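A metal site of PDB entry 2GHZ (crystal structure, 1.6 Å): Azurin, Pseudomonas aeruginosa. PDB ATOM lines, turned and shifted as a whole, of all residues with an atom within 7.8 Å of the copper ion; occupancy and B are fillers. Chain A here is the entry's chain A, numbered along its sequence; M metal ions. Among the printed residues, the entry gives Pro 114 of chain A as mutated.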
ATOM      1  N   GLY A   9      -0.518  29.534  14.045  1.00  0.00           N
ATOM      2  CA  GLY A   9      -1.092  28.208  13.768  1.00  0.00           C
ATOM      3  C   GLY A   9      -1.143  27.460  15.102  1.00  0.00           C
ATOM      4  O   GLY A   9      -0.153  27.375  15.769  1.00  0.00           O
ATOM      5  N   ASN A  10      -2.284  26.853  15.402  1.00  0.00           N
ATOM      6  CA  ASN A  10      -2.496  26.241  16.731  1.00  0.00           C
ATOM      7  C   ASN A  10      -2.520  24.706  16.700  1.00  0.00           C
ATOM      8  O   ASN A  10      -2.310  24.088  15.656  1.00  0.00           O
ATOM      9  CB  ASN A  10      -3.789  26.817  17.405  1.00  0.00           C
ATOM     10  CG  ASN A  10      -5.055  26.435  16.697  1.00  0.00           C
ATOM     11  OD1 ASN A  10      -5.073  25.538  15.875  1.00  0.00           O
ATOM     12  ND2 ASN A  10      -6.165  27.163  17.016  1.00  0.00           N
ATOM     13  N   MET A  13      -4.932  22.785  14.034  1.00  0.00           N
ATOM     14  CA  MET A  13      -4.743  22.914  12.570  1.00  0.00           C
ATOM     15  C   MET A  13      -5.577  24.104  12.036  1.00  0.00           C
ATOM     16  O   MET A  13      -6.265  24.022  11.003  1.00  0.00           O
ATOM     17  CB  MET A  13      -5.075  21.621  11.810  1.00  0.00           C
ATOM     18  CG  MET A  13      -4.280  20.384  12.246  1.00  0.00           C
ATOM     19  SD  MET A  13      -4.663  18.923  11.260  1.00  0.00           S
ATOM     20  CE  MET A  13      -6.359  18.656  11.750  1.00  0.00           C
ATOM     21  N   GLN A  14      -5.476  25.194  12.756  1.00  0.00           N
ATOM     22  CA  GLN A  14      -6.076  26.483  12.355  1.00  0.00           C
ATOM     23  C   GLN A  14      -5.050  27.606  12.295  1.00  0.00           C
ATOM     24  O   GLN A  14      -4.261  27.812  13.206  1.00  0.00           O
ATOM     25  CB  GLN A  14      -7.151  26.884  13.356  1.00  0.00           C
ATOM     26  CG  GLN A  14      -8.247  25.850  13.490  1.00  0.00           C
ATOM     27  CD  GLN A  14      -9.162  26.170  14.691  1.00  0.00           C
ATOM     28  OE1 GLN A  14      -8.840  27.054  15.516  1.00  0.00           O
ATOM     29  NE2 GLN A  14     -10.317  25.492  14.760  1.00  0.00           N
ATOM     30  N   PHE A  15      -5.060  28.333  11.199  1.00  0.00           N
ATOM     31  CA  PHE A  15      -4.460  29.666  11.204  1.00  0.00           C
ATOM     32  C   PHE A  15      -5.508  30.655  11.708  1.00  0.00           C
ATOM     33  O   PHE A  15      -6.725  30.443  11.504  1.00  0.00           O
ATOM     34  CB  PHE A  15      -4.131  30.118   9.789  1.00  0.00           C
ATOM     35  CG  PHE A  15      -2.843  29.583   9.200  1.00  0.00           C
ATOM     36  CD1 PHE A  15      -1.663  29.627   9.917  1.00  0.00           C
ATOM     37  CD2 PHE A  15      -2.812  29.142   7.906  1.00  0.00           C
ATOM     38  CE1 PHE A  15      -0.431  29.190   9.315  1.00  0.00           C
ATOM     39  CE2 PHE A  15      -1.622  28.700   7.301  1.00  0.00           C
ATOM     40  CZ  PHE A  15      -0.422  28.751   8.014  1.00  0.00           C
ATOM     41  N   HIS A  35       3.184  29.652  17.115  1.00  0.00           N
ATOM     42  CA  HIS A  35       2.448  28.377  17.281  1.00  0.00           C
ATOM     43  C   HIS A  35       1.985  28.208  18.717  1.00  0.00           C
ATOM     44  O   HIS A  35       2.654  27.517  19.521  1.00  0.00           O
ATOM     45  CB  HIS A  35       3.351  27.207  16.844  1.00  0.00           C
ATOM     46  CG  HIS A  35       2.674  25.879  16.766  1.00  0.00           C
ATOM     47  ND1 HIS A  35       1.642  25.479  17.595  1.00  0.00           N
ATOM     48  CD2 HIS A  35       2.957  24.812  15.979  1.00  0.00           C
ATOM     49  CE1 HIS A  35       1.311  24.226  17.290  1.00  0.00           C
ATOM     50  NE2 HIS A  35       2.120  23.799  16.322  1.00  0.00           N
ATOM     51  N   MET A  44       2.680  18.297  15.092  1.00  0.00           N
ATOM     52  CA  MET A  44       1.795  19.434  14.751  1.00  0.00           C
ATOM     53  C   MET A  44       2.627  20.647  14.327  1.00  0.00           C
ATOM     54  O   MET A  44       2.293  21.782  14.602  1.00  0.00           O
ATOM     55  CB  MET A  44       0.848  19.770  15.912  1.00  0.00           C
ATOM     56  CG  MET A  44      -0.303  20.716  15.564  1.00  0.00           C
ATOM     57  SD  MET A  44      -1.308  20.059  14.259  1.00  0.00           S
ATOM     58  CE  MET A  44      -2.057  18.643  15.033  1.00  0.00           C
ATOM     59  N   GLY A  45       3.738  20.395  13.642  1.00  0.00           N
ATOM     60  CA  GLY A  45       4.502  21.520  13.101  1.00  0.00           C
ATOM     61  C   GLY A  45       3.679  22.229  12.047  1.00  0.00           C
ATOM     62  O   GLY A  45       2.889  21.605  11.303  1.00  0.00           O
ATOM     63  N   HIS A  46       3.906  23.523  11.966  1.00  0.00           N
ATOM     64  CA  HIS A  46       3.272  24.377  10.938  1.00  0.00           C
ATOM     65  C   HIS A  46       4.338  25.213  10.231  1.00  0.00           C
ATOM     66  O   HIS A  46       5.358  25.610  10.804  1.00  0.00           O
ATOM     67  CB  HIS A  46       2.285  25.383  11.514  1.00  0.00           C
ATOM     68  CG  HIS A  46       1.156  24.760  12.258  1.00  0.00           C
ATOM     69  ND1 HIS A  46       0.359  23.781  11.723  1.00  0.00           N
ATOM     70  CD2 HIS A  46       0.662  25.017  13.497  1.00  0.00           C
ATOM     71  CE1 HIS A  46      -0.586  23.459  12.586  1.00  0.00           C
ATOM     72  NE2 HIS A  46      -0.397  24.176  13.680  1.00  0.00           N
ATOM     73  N   ASN A  47       4.034  25.546   8.988  1.00  0.00           N
ATOM     74  CA  ASN A  47       4.821  26.553   8.262  1.00  0.00           C
ATOM     75  C   ASN A  47       3.850  27.548   7.602  1.00  0.00           C
ATOM     76  O   ASN A  47       2.614  27.407   7.705  1.00  0.00           O
ATOM     77  CB  ASN A  47       5.793  25.907   7.255  1.00  0.00           C
ATOM     78  CG  ASN A  47       5.123  24.999   6.245  1.00  0.00           C
ATOM     79  OD1 ASN A  47       3.892  25.085   6.023  1.00  0.00           O
ATOM     80  ND2 ASN A  47       5.938  24.105   5.598  1.00  0.00           N
ATOM     81  N   TRP A  48       4.418  28.541   6.950  1.00  0.00           N
ATOM     82  CA  TRP A  48       3.645  29.504   6.186  1.00  0.00           C
ATOM     83  C   TRP A  48       4.333  29.572   4.813  1.00  0.00           C
ATOM     84  O   TRP A  48       5.509  29.907   4.708  1.00  0.00           O
ATOM     85  CB  TRP A  48       3.612  30.851   6.861  1.00  0.00           C
ATOM     86  CG  TRP A  48       2.745  31.884   6.158  1.00  0.00           C
ATOM     87  CD1 TRP A  48       1.423  32.133   6.378  1.00  0.00           C
ATOM     88  CD2 TRP A  48       3.156  32.790   5.113  1.00  0.00           C
ATOM     89  NE1 TRP A  48       0.994  33.171   5.563  1.00  0.00           N
ATOM     90  CE2 TRP A  48       2.024  33.553   4.748  1.00  0.00           C
ATOM     91  CE3 TRP A  48       4.353  32.998   4.413  1.00  0.00           C
ATOM     92  CZ2 TRP A  48       2.074  34.529   3.737  1.00  0.00           C
ATOM     93  CZ3 TRP A  48       4.370  33.950   3.412  1.00  0.00           C
ATOM     94  CH2 TRP A  48       3.243  34.707   3.110  1.00  0.00           C
ATOM     95  N   TYR A  72       8.518  19.600   4.982  1.00  0.00           N
ATOM     96  CA  TYR A  72       7.349  19.337   4.123  1.00  0.00           C
ATOM     97  C   TYR A  72       7.287  20.314   2.911  1.00  0.00           C
ATOM     98  O   TYR A  72       6.229  20.757   2.499  1.00  0.00           O
ATOM     99  CB  TYR A  72       6.068  19.374   4.896  1.00  0.00           C
ATOM    100  CG  TYR A  72       6.001  18.438   6.076  1.00  0.00           C
ATOM    101  CD1 TYR A  72       5.917  17.072   5.885  1.00  0.00           C
ATOM    102  CD2 TYR A  72       6.058  18.911   7.382  1.00  0.00           C
ATOM    103  CE1 TYR A  72       5.840  16.190   6.973  1.00  0.00           C
ATOM    104  CE2 TYR A  72       5.983  18.040   8.478  1.00  0.00           C
ATOM    105  CZ  TYR A  72       5.848  16.686   8.260  1.00  0.00           C
ATOM    106  OH  TYR A  72       5.747  15.801   9.321  1.00  0.00           O
ATOM    107  N   LEU A  86       9.450  25.296   9.265  1.00  0.00           N
ATOM    108  CA  LEU A  86       8.442  24.543  10.010  1.00  0.00           C
ATOM    109  C   LEU A  86       8.729  24.745  11.505  1.00  0.00           C
ATOM    110  O   LEU A  86       9.905  24.632  11.936  1.00  0.00           O
ATOM    111  CB  LEU A  86       8.608  23.054   9.665  1.00  0.00           C
ATOM    112  CG  LEU A  86       7.526  22.161  10.202  1.00  0.00           C
ATOM    113  CD1 LEU A  86       6.242  22.349   9.389  1.00  0.00           C
ATOM    114  CD2 LEU A  86       7.965  20.715  10.172  1.00  0.00           C
ATOM    115  N   ILE A  87       7.696  25.048  12.283  1.00  0.00           N
ATOM    116  CA  ILE A  87       7.866  25.332  13.695  1.00  0.00           C
ATOM    117  C   ILE A  87       6.899  24.453  14.552  1.00  0.00           C
ATOM    118  O   ILE A  87       5.788  24.154  14.125  1.00  0.00           O
ATOM    119  CB  ILE A  87       7.662  26.829  14.052  1.00  0.00           C
ATOM    120  CG1 ILE A  87       6.210  27.275  13.776  1.00  0.00           C
ATOM    121  CG2 ILE A  87       8.626  27.683  13.314  1.00  0.00           C
ATOM    122  CD1 ILE A  87       5.917  28.610  14.323  1.00  0.00           C
ATOM    123  N   PHE A 111      -0.537  28.973   2.772  1.00  0.00           N
ATOM    124  CA  PHE A 111      -0.978  27.670   3.276  1.00  0.00           C
ATOM    125  C   PHE A 111       0.124  27.016   4.064  1.00  0.00           C
ATOM    126  O   PHE A 111       1.259  27.441   4.009  1.00  0.00           O
ATOM    127  CB  PHE A 111      -1.454  26.779   2.143  1.00  0.00           C
ATOM    128  CG  PHE A 111      -0.526  26.765   0.970  1.00  0.00           C
ATOM    129  CD1 PHE A 111      -0.602  27.756  -0.006  1.00  0.00           C
ATOM    130  CD2 PHE A 111       0.464  25.808   0.848  1.00  0.00           C
ATOM    131  CE1 PHE A 111       0.234  27.791  -1.064  1.00  0.00           C
ATOM    132  CE2 PHE A 111       1.335  25.821  -0.240  1.00  0.00           C
ATOM    133  CZ  PHE A 111       1.239  26.800  -1.191  1.00  0.00           C
ATOM    134  N   CYS A 112      -0.295  25.996   4.826  1.00  0.00           N
ATOM    135  CA  CYS A 112       0.582  25.188   5.656  1.00  0.00           C
ATOM    136  C   CYS A 112       0.705  23.820   4.994  1.00  0.00           C
ATOM    137  O   CYS A 112      -0.294  23.173   4.748  1.00  0.00           O
ATOM    138  CB  CYS A 112      -0.026  25.032   7.058  1.00  0.00           C
ATOM    139  SG  CYS A 112       1.088  24.496   8.284  1.00  0.00           S
ATOM    140  N   THR A 113       1.908  23.393   4.600  1.00  0.00           N
ATOM    141  CA  THR A 113       2.060  22.157   3.804  1.00  0.00           C
ATOM    142  C   THR A 113       2.088  20.791   4.514  1.00  0.00           C
ATOM    143  O   THR A 113       2.003  19.779   3.828  1.00  0.00           O
ATOM    144  CB  THR A 113       3.303  22.218   2.893  1.00  0.00           C
ATOM    145  OG1 THR A 113       4.468  22.358   3.705  1.00  0.00           O
ATOM    146  CG2 THR A 113       3.184  23.443   1.915  1.00  0.00           C
ATOM    147  N   PRO A 114       2.276  20.751   5.836  1.00  0.00           N
ATOM    148  CA  PRO A 114       2.289  19.410   6.461  1.00  0.00           C
ATOM    149  C   PRO A 114       1.093  18.522   6.167  1.00  0.00           C
ATOM    150  O   PRO A 114      -0.036  18.999   6.005  1.00  0.00           O
ATOM    151  CB  PRO A 114       2.375  19.693   7.956  1.00  0.00           C
ATOM    152  CG  PRO A 114       3.076  21.024   8.061  1.00  0.00           C
ATOM    153  CD  PRO A 114       2.689  21.797   6.790  1.00  0.00           C
ATOM    154  N   PRO A 115       1.334  17.191   6.202  1.00  0.00           N
ATOM    155  CA  PRO A 115       0.288  16.231   6.006  1.00  0.00           C
ATOM    156  C   PRO A 115      -0.963  16.558   6.797  1.00  0.00           C
ATOM    157  O   PRO A 115      -0.915  16.783   8.011  1.00  0.00           O
ATOM    158  CB  PRO A 115       0.929  14.946   6.503  1.00  0.00           C
ATOM    159  CG  PRO A 115       2.344  15.103   6.125  1.00  0.00           C
ATOM    160  CD  PRO A 115       2.643  16.559   6.392  1.00  0.00           C
ATOM    161  N   GLY A 116      -2.072  16.630   6.088  1.00  0.00           N
ATOM    162  CA  GLY A 116      -3.356  16.876   6.685  1.00  0.00           C
ATOM    163  C   GLY A 116      -3.713  18.318   6.930  1.00  0.00           C
ATOM    164  O   GLY A 116      -4.883  18.621   7.253  1.00  0.00           O
ATOM    165  N   HIS A 117      -2.772  19.249   6.745  1.00  0.00           N
ATOM    166  CA  HIS A 117      -3.018  20.648   7.150  1.00  0.00           C
ATOM    167  C   HIS A 117      -3.510  21.600   6.052  1.00  0.00           C
ATOM    168  O   HIS A 117      -4.209  22.544   6.354  1.00  0.00           O
ATOM    169  CB  HIS A 117      -1.745  21.270   7.735  1.00  0.00           C
ATOM    170  CG  HIS A 117      -1.278  20.665   9.022  1.00  0.00           C
ATOM    171  ND1 HIS A 117      -0.536  21.378   9.949  1.00  0.00           N
ATOM    172  CD2 HIS A 117      -1.450  19.424   9.559  1.00  0.00           C
ATOM    173  CE1 HIS A 117      -0.275  20.602  10.990  1.00  0.00           C
ATOM    174  NE2 HIS A 117      -0.801  19.407  10.772  1.00  0.00           N
ATOM    175  N   SER A 118      -3.061  21.380   4.811  1.00  0.00           N
ATOM    176  CA  SER A 118      -3.209  22.448   3.808  1.00  0.00           C
ATOM    177  C   SER A 118      -4.665  22.771   3.485  1.00  0.00           C
ATOM    178  O   SER A 118      -4.999  23.934   3.198  1.00  0.00           O
ATOM    179  CB  SER A 118      -2.444  22.132   2.523  1.00  0.00           C
ATOM    180  OG  SER A 118      -3.003  21.030   1.827  1.00  0.00           O
ATOM    181  N   LEU A 120      -7.049  22.741   5.554  1.00  0.00           N
ATOM    182  CA  LEU A 120      -7.559  23.354   6.753  1.00  0.00           C
ATOM    183  C   LEU A 120      -6.856  24.660   7.120  1.00  0.00           C
ATOM    184  O   LEU A 120      -7.325  25.419   7.985  1.00  0.00           O
ATOM    185  CB  LEU A 120      -7.387  22.393   7.927  1.00  0.00           C
ATOM    186  CG  LEU A 120      -8.181  21.076   7.780  1.00  0.00           C
ATOM    187  CD1 LEU A 120      -7.805  20.131   8.923  1.00  0.00           C
ATOM    188  CD2 LEU A 120      -9.656  21.323   7.795  1.00  0.00           C
ATOM    189  N   MET A 121      -5.729  24.919   6.462  1.00  0.00           N
ATOM    190  CA  MET A 121      -4.810  25.975   6.862  1.00  0.00           C
ATOM    191  C   MET A 121      -4.321  26.676   5.601  1.00  0.00           C
ATOM    192  O   MET A 121      -3.224  26.476   5.092  1.00  0.00           O
ATOM    193  CB  MET A 121      -3.587  25.423   7.675  1.00  0.00           C
ATOM    194  CG  MET A 121      -4.001  24.875   9.018  1.00  0.00           C
ATOM    195  SD  MET A 121      -2.625  24.411  10.091  1.00  0.00           S
ATOM    196  CE  MET A 121      -2.043  26.006  10.601  1.00  0.00           C
HETATM  197 CU    CU M   1       0.100  23.239   9.748  1.00  0.00          CU
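The copper ion is bound by a ring nitrogen (ND1) of His 117 (2.0 Å), a ring nitrogen (ND1) of His 46 (2.1 Å) and the side-chain sulfur of Cys 112 (2.2 Å). Slightly farther from the copper ion lies the side-chain sulfur (SD) of Met 121 (3.0 Å).
ND1 of His 117 lies close to SD of Met 121, 3.7 Å away. SD of Met 44 sits close to NE2 of His 117. The side-chain sulfur (SD) of Met 121 sits close to a ring nitrogen (ND1) of His 46 (3.5 Å). The backbone carbonyl oxygen of Asn 10 is in hydrogen-bond range of a ring nitrogen (NE2) of His 46, at 2.8 Å. O of His 46 sits at hydrogen-bond distance from N of Ile 87, 2.8 Å away. N of Cys 112 is in hydrogen-bond range of O of Met 121 (3.0 Å). The side-chain sulfur (SG) of Cys 112 lies close to the backbone NH (N) of Asn 47 (3.2 Å). O of Cys 112 lies close to N of Ser 118 (3.3 Å).
Gly 45 touches the copper ion (O to CU, 3.6 Å). Of the 24 residues printed, 5 come within 4 Å of the copper ion. The nearest printed residue that does not touch the copper ion is Pro 114 (4.1 Å).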
